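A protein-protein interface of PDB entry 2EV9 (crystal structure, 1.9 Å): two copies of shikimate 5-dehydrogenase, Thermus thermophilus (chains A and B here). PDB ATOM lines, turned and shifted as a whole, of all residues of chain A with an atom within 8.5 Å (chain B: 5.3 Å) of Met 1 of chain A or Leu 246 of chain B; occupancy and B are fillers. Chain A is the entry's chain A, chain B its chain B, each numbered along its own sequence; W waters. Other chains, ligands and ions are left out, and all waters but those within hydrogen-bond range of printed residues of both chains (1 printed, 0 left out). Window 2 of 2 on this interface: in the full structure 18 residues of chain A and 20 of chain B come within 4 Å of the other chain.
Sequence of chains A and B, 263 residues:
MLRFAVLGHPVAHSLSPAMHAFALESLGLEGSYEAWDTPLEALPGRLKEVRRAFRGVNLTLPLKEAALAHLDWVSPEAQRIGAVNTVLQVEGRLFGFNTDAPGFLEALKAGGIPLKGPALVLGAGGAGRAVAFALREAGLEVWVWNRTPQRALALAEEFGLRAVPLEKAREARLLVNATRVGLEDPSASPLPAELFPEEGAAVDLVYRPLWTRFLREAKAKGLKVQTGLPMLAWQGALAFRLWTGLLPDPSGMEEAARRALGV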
ATOM      1  N   MET A   1      -3.736 -28.212  15.551  1.00  0.00           N
ATOM      2  CA  MET A   1      -4.176 -26.827  15.208  1.00  0.00           C
ATOM      3  C   MET A   1      -5.676 -26.771  14.923  1.00  0.00           C
ATOM      4  O   MET A   1      -6.242 -25.691  14.731  1.00  0.00           O
ATOM      5  CB  MET A   1      -3.389 -26.311  13.997  1.00  0.00           C
ATOM      6  CG  MET A   1      -3.598 -27.104  12.720  1.00  0.00           C
ATOM      7  SD  MET A   1      -2.272 -26.810  11.515  1.00  0.00           S
ATOM      8  CE  MET A   1      -2.630 -25.125  11.034  1.00  0.00           C
ATOM      9  N   LEU A   2      -6.309 -27.941  14.898  1.00  0.00           N
ATOM     10  CA  LEU A   2      -7.743 -28.060  14.647  1.00  0.00           C
ATOM     11  C   LEU A   2      -8.513 -27.708  15.910  1.00  0.00           C
ATOM     12  O   LEU A   2      -8.534 -28.481  16.871  1.00  0.00           O
ATOM     13  CB  LEU A   2      -8.086 -29.490  14.232  1.00  0.00           C
ATOM     14  CG  LEU A   2      -7.504 -29.951  12.895  1.00  0.00           C
ATOM     15  CD1 LEU A   2      -7.779 -31.440  12.679  1.00  0.00           C
ATOM     16  CD2 LEU A   2      -8.116 -29.122  11.790  1.00  0.00           C
ATOM     17  N   ARG A   3      -9.151 -26.545  15.908  1.00  0.00           N
ATOM     18  CA  ARG A   3      -9.904 -26.110  17.075  1.00  0.00           C
ATOM     19  C   ARG A   3     -11.402 -26.223  16.832  1.00  0.00           C
ATOM     20  O   ARG A   3     -11.943 -25.540  15.965  1.00  0.00           O
ATOM     21  CB  ARG A   3      -9.531 -24.664  17.426  1.00  0.00           C
ATOM     22  CG  ARG A   3      -9.758 -24.330  18.884  1.00  0.00           C
ATOM     23  CD  ARG A   3      -9.211 -22.955  19.250  1.00  0.00           C
ATOM     24  NE  ARG A   3      -9.049 -22.828  20.696  1.00  0.00           N
ATOM     25  CZ  ARG A   3      -8.151 -23.508  21.408  1.00  0.00           C
ATOM     26  NH1 ARG A   3      -7.326 -24.359  20.807  1.00  0.00           N
ATOM     27  NH2 ARG A   3      -8.092 -23.359  22.727  1.00  0.00           N
ATOM     28  N   PHE A   4     -12.053 -27.092  17.603  1.00  0.00           N
ATOM     29  CA  PHE A   4     -13.493 -27.333  17.488  1.00  0.00           C
ATOM     30  C   PHE A   4     -14.196 -27.145  18.833  1.00  0.00           C
ATOM     31  O   PHE A   4     -13.550 -26.988  19.862  1.00  0.00           O
ATOM     32  CB  PHE A   4     -13.763 -28.761  17.019  1.00  0.00           C
ATOM     33  CG  PHE A   4     -13.134 -29.106  15.709  1.00  0.00           C
ATOM     34  CD1 PHE A   4     -12.148 -30.086  15.637  1.00  0.00           C
ATOM     35  CD2 PHE A   4     -13.547 -28.484  14.539  1.00  0.00           C
ATOM     36  CE1 PHE A   4     -11.583 -30.445  14.415  1.00  0.00           C
ATOM     37  CE2 PHE A   4     -12.986 -28.834  13.309  1.00  0.00           C
ATOM     38  CZ  PHE A   4     -12.003 -29.817  13.250  1.00  0.00           C
ATOM     39  N   LEU A  24      -9.939 -37.245  16.655  1.00  0.00           N
ATOM     40  CA  LEU A  24      -8.632 -36.635  16.453  1.00  0.00           C
ATOM     41  C   LEU A  24      -7.520 -37.654  16.691  1.00  0.00           C
ATOM     42  O   LEU A  24      -6.677 -37.890  15.821  1.00  0.00           O
ATOM     43  CB  LEU A  24      -8.466 -35.445  17.395  1.00  0.00           C
ATOM     44  CG  LEU A  24      -9.311 -34.213  17.054  1.00  0.00           C
ATOM     45  CD1 LEU A  24      -9.345 -33.261  18.229  1.00  0.00           C
ATOM     46  CD2 LEU A  24      -8.743 -33.525  15.818  1.00  0.00           C
ATOM     47  N   LEU A  27      -7.251 -40.560  14.287  1.00  0.00           N
ATOM     48  CA  LEU A  27      -6.800 -40.134  12.965  1.00  0.00           C
ATOM     49  C   LEU A  27      -5.407 -39.508  13.006  1.00  0.00           C
ATOM     50  O   LEU A  27      -4.961 -38.902  12.031  1.00  0.00           O
ATOM     51  CB  LEU A  27      -7.786 -39.130  12.368  1.00  0.00           C
ATOM     52  CG  LEU A  27      -9.191 -39.639  12.058  1.00  0.00           C
ATOM     53  CD1 LEU A  27     -10.072 -38.470  11.637  1.00  0.00           C
ATOM     54  CD2 LEU A  27      -9.125 -40.692  10.954  1.00  0.00           C
ATOM     55  N   GLY A  28      -4.731 -39.645  14.140  1.00  0.00           N
ATOM     56  CA  GLY A  28      -3.397 -39.095  14.269  1.00  0.00           C
ATOM     57  C   GLY A  28      -3.345 -37.600  14.035  1.00  0.00           C
ATOM     58  O   GLY A  28      -2.354 -37.082  13.516  1.00  0.00           O
ATOM     59  N   LEU A  29      -4.412 -36.905  14.414  1.00  0.00           N
ATOM     60  CA  LEU A  29      -4.483 -35.455  14.242  1.00  0.00           C
ATOM     61  C   LEU A  29      -4.342 -34.740  15.581  1.00  0.00           C
ATOM     62  O   LEU A  29      -4.719 -35.273  16.623  1.00  0.00           O
ATOM     63  CB  LEU A  29      -5.824 -35.056  13.613  1.00  0.00           C
ATOM     64  CG  LEU A  29      -6.176 -35.607  12.230  1.00  0.00           C
ATOM     65  CD1 LEU A  29      -7.628 -35.271  11.898  1.00  0.00           C
ATOM     66  CD2 LEU A  29      -5.230 -35.027  11.190  1.00  0.00           C
ATOM     67  N   GLU A  30      -3.790 -33.533  15.544  1.00  0.00           N
ATOM     68  CA  GLU A  30      -3.624 -32.725  16.743  1.00  0.00           C
ATOM     69  C   GLU A  30      -4.712 -31.663  16.744  1.00  0.00           C
ATOM     70  O   GLU A  30      -4.888 -30.941  15.768  1.00  0.00           O
ATOM     71  CB  GLU A  30      -2.246 -32.054  16.761  1.00  0.00           C
ATOM     72  CG  GLU A  30      -1.215 -32.768  17.623  1.00  0.00           C
ATOM     73  CD  GLU A  30      -1.678 -32.943  19.064  1.00  0.00           C
ATOM     74  OE1 GLU A  30      -2.278 -31.996  19.618  1.00  0.00           O
ATOM     75  OE2 GLU A  30      -1.433 -34.023  19.645  1.00  0.00           O
ATOM     76  N   GLY A  31      -5.449 -31.581  17.840  1.00  0.00           N
ATOM     77  CA  GLY A  31      -6.513 -30.606  17.930  1.00  0.00           C
ATOM     78  C   GLY A  31      -7.276 -30.737  19.230  1.00  0.00           C
ATOM     79  O   GLY A  31      -6.890 -31.493  20.120  1.00  0.00           O
ATOM     80  N   SER A  32      -8.373 -30.005  19.335  1.00  0.00           N
ATOM     81  CA  SER A  32      -9.180 -30.031  20.542  1.00  0.00           C
ATOM     82  C   SER A  32     -10.651 -29.811  20.226  1.00  0.00           C
ATOM     83  O   SER A  32     -10.999 -29.246  19.187  1.00  0.00           O
ATOM     84  CB  SER A  32      -8.699 -28.943  21.510  1.00  0.00           C
ATOM     85  OG  SER A  32      -8.784 -27.665  20.901  1.00  0.00           O
ATOM     86  N   ALA A  53     -11.065 -18.066  15.516  1.00  0.00           N
ATOM     87  CA  ALA A  53     -10.215 -19.148  15.994  1.00  0.00           C
ATOM     88  C   ALA A  53     -10.759 -20.569  15.915  1.00  0.00           C
ATOM     89  O   ALA A  53     -10.157 -21.484  16.477  1.00  0.00           O
ATOM     90  CB  ALA A  53      -9.777 -18.848  17.430  1.00  0.00           C
ATOM     91  N   PHE A  54     -11.879 -20.773  15.230  1.00  0.00           N
ATOM     92  CA  PHE A  54     -12.420 -22.125  15.131  1.00  0.00           C
ATOM     93  C   PHE A  54     -12.625 -22.612  13.707  1.00  0.00           C
ATOM     94  O   PHE A  54     -13.168 -21.904  12.857  1.00  0.00           O
ATOM     95  CB  PHE A  54     -13.741 -22.243  15.903  1.00  0.00           C
ATOM     96  CG  PHE A  54     -13.579 -22.171  17.395  1.00  0.00           C
ATOM     97  CD1 PHE A  54     -13.325 -20.955  18.024  1.00  0.00           C
ATOM     98  CD2 PHE A  54     -13.651 -23.324  18.171  1.00  0.00           C
ATOM     99  CE1 PHE A  54     -13.143 -20.891  19.408  1.00  0.00           C
ATOM    100  CE2 PHE A  54     -13.470 -23.272  19.555  1.00  0.00           C
ATOM    101  CZ  PHE A  54     -13.216 -22.052  20.172  1.00  0.00           C
ATOM    102  N   ARG A  55     -12.168 -23.831  13.452  1.00  0.00           N
ATOM    103  CA  ARG A  55     -12.319 -24.443  12.142  1.00  0.00           C
ATOM    104  C   ARG A  55     -13.787 -24.831  11.949  1.00  0.00           C
ATOM    105  O   ARG A  55     -14.324 -24.766  10.841  1.00  0.00           O
ATOM    106  CB  ARG A  55     -11.443 -25.693  12.043  1.00  0.00           C
ATOM    107  CG  ARG A  55     -11.740 -26.564  10.832  1.00  0.00           C
ATOM    108  CD  ARG A  55     -11.395 -25.873   9.524  1.00  0.00           C
ATOM    109  NE  ARG A  55     -11.614 -26.764   8.384  1.00  0.00           N
ATOM    110  CZ  ARG A  55     -11.349 -26.444   7.121  1.00  0.00           C
ATOM    111  NH1 ARG A  55     -10.851 -25.253   6.827  1.00  0.00           N
ATOM    112  NH2 ARG A  55     -11.586 -27.316   6.152  1.00  0.00           N
ATOM    113  N   GLY A  56     -14.429 -25.237  13.040  1.00  0.00           N
ATOM    114  CA  GLY A  56     -15.825 -25.623  12.967  1.00  0.00           C
ATOM    115  C   GLY A  56     -16.439 -25.874  14.329  1.00  0.00           C
ATOM    116  O   GLY A  56     -15.734 -26.079  15.321  1.00  0.00           O
ATOM    117  N   TRP A 243     -15.585 -30.944   8.265  1.00  0.00           N
ATOM    118  CA  TRP A 243     -14.498 -30.068   8.670  1.00  0.00           C
ATOM    119  C   TRP A 243     -13.116 -30.410   8.120  1.00  0.00           C
ATOM    120  O   TRP A 243     -12.348 -29.515   7.781  1.00  0.00           O
ATOM    121  CB  TRP A 243     -14.388 -30.021  10.206  1.00  0.00           C
ATOM    122  CG  TRP A 243     -15.600 -29.509  10.924  1.00  0.00           C
ATOM    123  CD1 TRP A 243     -16.449 -28.524  10.503  1.00  0.00           C
ATOM    124  CD2 TRP A 243     -16.084 -29.937  12.199  1.00  0.00           C
ATOM    125  NE1 TRP A 243     -17.433 -28.316  11.439  1.00  0.00           N
ATOM    126  CE2 TRP A 243     -17.233 -29.169  12.490  1.00  0.00           C
ATOM    127  CE3 TRP A 243     -15.659 -30.894  13.128  1.00  0.00           C
ATOM    128  CZ2 TRP A 243     -17.964 -29.332  13.669  1.00  0.00           C
ATOM    129  CZ3 TRP A 243     -16.388 -31.056  14.301  1.00  0.00           C
ATOM    130  CH2 TRP A 243     -17.530 -30.278  14.559  1.00  0.00           C
ATOM    131  N   THR A 244     -12.804 -31.697   8.029  1.00  0.00           N
ATOM    132  CA  THR A 244     -11.466 -32.118   7.614  1.00  0.00           C
ATOM    133  C   THR A 244     -11.316 -32.914   6.331  1.00  0.00           C
ATOM    134  O   THR A 244     -10.225 -32.957   5.752  1.00  0.00           O
ATOM    135  CB  THR A 244     -10.817 -32.969   8.709  1.00  0.00           C
ATOM    136  OG1 THR A 244     -11.506 -34.227   8.803  1.00  0.00           O
ATOM    137  CG2 THR A 244     -10.897 -32.258  10.053  1.00  0.00           C
ATOM    138  N   LEU A 246     -11.884 -35.999   6.454  1.00  0.00           N
ATOM    139  CA  LEU A 246     -11.626 -37.328   7.018  1.00  0.00           C
ATOM    140  C   LEU A 246     -12.823 -37.844   7.816  1.00  0.00           C
ATOM    141  O   LEU A 246     -13.436 -37.094   8.583  1.00  0.00           O
ATOM    142  CB  LEU A 246     -10.401 -37.276   7.935  1.00  0.00           C
ATOM    143  CG  LEU A 246      -9.089 -36.832   7.287  1.00  0.00           C
ATOM    144  CD1 LEU A 246      -8.061 -36.528   8.359  1.00  0.00           C
ATOM    145  CD2 LEU A 246      -8.600 -37.924   6.347  1.00  0.00           C
ATOM    146  N   LEU B  27       2.355 -33.843   6.869  1.00  0.00           N
ATOM    147  CA  LEU B  27       1.255 -33.783   7.826  1.00  0.00           C
ATOM    148  C   LEU B  27       0.772 -35.181   8.205  1.00  0.00           C
ATOM    149  O   LEU B  27      -0.169 -35.333   8.988  1.00  0.00           O
ATOM    150  CB  LEU B  27       0.099 -32.959   7.247  1.00  0.00           C
ATOM    151  CG  LEU B  27       0.389 -31.465   7.051  1.00  0.00           C
ATOM    152  CD1 LEU B  27      -0.732 -30.817   6.272  1.00  0.00           C
ATOM    153  CD2 LEU B  27       0.553 -30.788   8.407  1.00  0.00           C
ATOM    154  N   LEU B  29      -0.773 -37.353   6.352  1.00  0.00           N
ATOM    155  CA  LEU B  29      -2.106 -37.581   5.805  1.00  0.00           C
ATOM    156  C   LEU B  29      -2.047 -38.461   4.563  1.00  0.00           C
ATOM    157  O   LEU B  29      -1.103 -38.375   3.777  1.00  0.00           O
ATOM    158  CB  LEU B  29      -2.765 -36.247   5.442  1.00  0.00           C
ATOM    159  CG  LEU B  29      -3.084 -35.280   6.582  1.00  0.00           C
ATOM    160  CD1 LEU B  29      -3.524 -33.952   5.995  1.00  0.00           C
ATOM    161  CD2 LEU B  29      -4.178 -35.855   7.468  1.00  0.00           C
ATOM    162  N   ALA B 237      -0.495 -23.442   0.447  1.00  0.00           N
ATOM    163  CA  ALA B 237      -0.619 -23.844   1.843  1.00  0.00           C
ATOM    164  C   ALA B 237      -1.966 -23.359   2.364  1.00  0.00           C
ATOM    165  O   ALA B 237      -2.638 -24.045   3.138  1.00  0.00           O
ATOM    166  CB  ALA B 237       0.516 -23.241   2.672  1.00  0.00           C
ATOM    167  N   PHE B 240      -4.594 -25.688   1.106  1.00  0.00           N
ATOM    168  CA  PHE B 240      -4.617 -26.955   1.835  1.00  0.00           C
ATOM    169  C   PHE B 240      -5.346 -26.769   3.170  1.00  0.00           C
ATOM    170  O   PHE B 240      -6.143 -27.621   3.587  1.00  0.00           O
ATOM    171  CB  PHE B 240      -3.192 -27.453   2.094  1.00  0.00           C
ATOM    172  CG  PHE B 240      -3.116 -28.925   2.387  1.00  0.00           C
ATOM    173  CD1 PHE B 240      -3.009 -29.851   1.347  1.00  0.00           C
ATOM    174  CD2 PHE B 240      -3.208 -29.392   3.692  1.00  0.00           C
ATOM    175  CE1 PHE B 240      -2.998 -31.220   1.606  1.00  0.00           C
ATOM    176  CE2 PHE B 240      -3.199 -30.768   3.968  1.00  0.00           C
ATOM    177  CZ  PHE B 240      -3.095 -31.682   2.924  1.00  0.00           C
ATOM    178  N   ARG B 241      -5.079 -25.655   3.846  1.00  0.00           N
ATOM    179  CA  ARG B 241      -5.743 -25.408   5.124  1.00  0.00           C
ATOM    180  C   ARG B 241      -7.241 -25.285   4.876  1.00  0.00           C
ATOM    181  O   ARG B 241      -8.059 -25.811   5.628  1.00  0.00           O
ATOM    182  CB  ARG B 241      -5.232 -24.121   5.785  1.00  0.00           C
ATOM    183  CG  ARG B 241      -5.790 -23.934   7.195  1.00  0.00           C
ATOM    184  CD  ARG B 241      -5.396 -22.613   7.815  1.00  0.00           C
ATOM    185  NE  ARG B 241      -6.002 -21.495   7.104  1.00  0.00           N
ATOM    186  CZ  ARG B 241      -5.848 -20.222   7.443  1.00  0.00           C
ATOM    187  NH1 ARG B 241      -5.105 -19.901   8.493  1.00  0.00           N
ATOM    188  NH2 ARG B 241      -6.427 -19.270   6.724  1.00  0.00           N
ATOM    189  N   THR B 244      -8.574 -28.798   4.544  1.00  0.00           N
ATOM    190  CA  THR B 244      -8.487 -29.677   5.700  1.00  0.00           C
ATOM    191  C   THR B 244      -8.450 -29.045   7.082  1.00  0.00           C
ATOM    192  O   THR B 244      -8.725 -29.714   8.080  1.00  0.00           O
ATOM    193  CB  THR B 244      -7.239 -30.554   5.573  1.00  0.00           C
ATOM    194  OG1 THR B 244      -6.074 -29.751   5.810  1.00  0.00           O
ATOM    195  CG2 THR B 244      -7.140 -31.127   4.171  1.00  0.00           C
ATOM    196  N   GLY B 245      -8.104 -27.768   7.147  1.00  0.00           N
ATOM    197  CA  GLY B 245      -8.010 -27.110   8.431  1.00  0.00           C
ATOM    198  C   GLY B 245      -6.579 -27.178   8.938  1.00  0.00           C
ATOM    199  O   GLY B 245      -6.259 -26.660  10.009  1.00  0.00           O
ATOM    200  N   LEU B 246      -5.717 -27.826   8.161  1.00  0.00           N
ATOM    201  CA  LEU B 246      -4.313 -27.968   8.515  1.00  0.00           C
ATOM    202  C   LEU B 246      -3.443 -27.147   7.565  1.00  0.00           C
ATOM    203  O   LEU B 246      -3.613 -27.209   6.342  1.00  0.00           O
ATOM    204  CB  LEU B 246      -3.897 -29.438   8.438  1.00  0.00           C
ATOM    205  CG  LEU B 246      -4.519 -30.416   9.436  1.00  0.00           C
ATOM    206  CD1 LEU B 246      -3.925 -31.798   9.212  1.00  0.00           C
ATOM    207  CD2 LEU B 246      -4.244 -29.950  10.856  1.00  0.00           C
ATOM    208  N   LEU B 247      -2.512 -26.382   8.130  1.00  0.00           N
ATOM    209  CA  LEU B 247      -1.611 -25.552   7.334  1.00  0.00           C
ATOM    210  C   LEU B 247      -0.254 -26.217   7.193  1.00  0.00           C
ATOM    211  O   LEU B 247       0.467 -26.381   8.179  1.00  0.00           O
ATOM    212  CB  LEU B 247      -1.406 -24.173   7.984  1.00  0.00           C
ATOM    213  CG  LEU B 247      -0.374 -23.255   7.300  1.00  0.00           C
ATOM    214  CD1 LEU B 247      -0.973 -22.619   6.048  1.00  0.00           C
ATOM    215  CD2 LEU B 247       0.068 -22.155   8.265  1.00  0.00           C
ATOM    216  N   PRO B 248       0.106 -26.634   5.971  1.00  0.00           N
ATOM    217  CA  PRO B 248       1.417 -27.264   5.806  1.00  0.00           C
ATOM    218  C   PRO B 248       2.487 -26.170   5.855  1.00  0.00           C
ATOM    219  O   PRO B 248       2.196 -24.995   5.599  1.00  0.00           O
ATOM    220  CB  PRO B 248       1.309 -27.933   4.439  1.00  0.00           C
ATOM    221  CG  PRO B 248       0.380 -27.024   3.697  1.00  0.00           C
ATOM    222  CD  PRO B 248      -0.674 -26.686   4.721  1.00  0.00           C
HETATM  223  O   HOH W   1      -1.273 -34.682  11.294  1.00  0.00           O
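The side-chain sulfur (SD) of Met 1 of chain A sits close to the backbone NH (N) of Leu 247 of chain B.
The backbone carbonyl oxygen of Arg 241 of chain B sits at hydrogen-bond distance from the guanidinium group of Arg 55 of chain A (3.1 Å).
N of Leu 246 of chain A sits at hydrogen-bond distance from OG1 of Thr 244 of chain A (3.0 Å).
The guanidinium group (NH2) of Arg 55 of chain A sits at hydrogen-bond distance from the backbone carbonyl oxygen (O) of Trp 243 of chain A, 2.8 Å away.
The backbone carbonyl oxygen (O) of Arg 3 of chain A lies within hydrogen-bond range of the backbone NH (N) of Arg 55 of chain A (3.0 Å).
The backbone NH (N) of Met 1 of chain A lies within hydrogen-bond range of the backbone carbonyl oxygen (O) of Glu 30 of chain A (3.0 Å).
O of Leu 246 of chain B lies close to N of Arg 241 of chain B (3.3 Å).
The backbone NH (N) of Leu 2 of chain A lies within hydrogen-bond range of the backbone carbonyl oxygen (O) of Glu 30 of chain A (3.4 Å).
Among the printed residues, pairs that only touch across the chains: Met 1 of chain A with Leu 246 of chain B (3.5 Å), Arg 55 of chain A with Gly 245 of chain B (3.5 Å), Leu 2 of chain A with Gly 245 of chain B (3.6 Å), Trp 243 of chain A with Thr 244 of chain B (3.6 Å), Thr 244 of chain A with Thr 244 of chain B (3.7 Å), Arg 55 of chain A with Thr 244 of chain B (3.7 Å), Leu 2 of chain A with Thr 244 of chain B (3.8 Å), Met 1 of chain A with Gly 245 of chain B (3.8 Å), Leu 2 of chain A with Leu 246 of chain B (3.8 Å) and Leu 29 of chain A with Leu 29 of chain B (3.96 Å).
Of chain B, only Gly 245 (3.8 Å), Leu 246 (3.5 Å) and Leu 247 (3.2 Å) come within 4 Å of Met 1 of chain A.
Printed residues of chain B within 4 Å of Leu 2 of chain A: Thr 244 (3.8 Å), Gly 245 (3.6 Å) and Leu 246 (3.8 Å).
Of the printed residues of chain B, Arg 55 of chain A touches Arg 241, Thr 244 and Gly 245.
Printed residues of chain B within 4 Å of Trp 243 of chain A: Thr 244.
Phe 240 of chain B touches none of the printed residues of chain A.
Of the printed residues of chain A, Arg 241 of chain B touches Arg 55 (3.1 Å).
Printed residues of chain A within 4 Å of Thr 244 of chain B: Leu 2, Arg 55, Trp 243 and Thr 244.
Gly 245 of chain B touches just these residues of chain A: Met 1 (3.8 Å), Leu 2 (3.6 Å) and Arg 55 (3.5 Å).
Of the printed residues of chain A, Leu 246 of chain B touches Met 1 (3.5 Å) and Leu 2 (3.8 Å).
Pro 248 of chain B touches none of the printed residues of chain A.
The nearest residue of chain B that does not touch Met 1 of chain A is Arg 241 of chain B (4.9 Å).
The nearest printed residue of chain A that does not touch Leu 246 of chain B is Leu 29 of chain A (4.01 Å).
The nearest printed residue of chain B that does not touch Arg 55 of chain A is Leu 246 of chain B (5.9 Å).
Printed residues of chain B that touch a printed residue of chain A: Leu 29, Arg 241, Thr 244, Gly 245, Leu 246 and Leu 247.
Printed residues of chain A that touch a printed residue of chain B: Met 1, Leu 2, Leu 29, Arg 55, Trp 243 and Thr 244.
Among the printed residues, 12 pairs touch across the chains.
Leu 29 of chain B touches its own counterpart, Leu 29 of chain A.
Thr 244 of chain B touches its own counterpart, Thr 244 of chain A.
4 positions are printed for both chains.
Of the 12 pairs that touch across the chains among the printed residues, 2 have their exchanged pair printed and touching as well.
Water W1 lies within hydrogen-bond range of O of Leu 27 of chain B (2.6 Å) and O of Gly 28 of chain A (3.4 Å).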
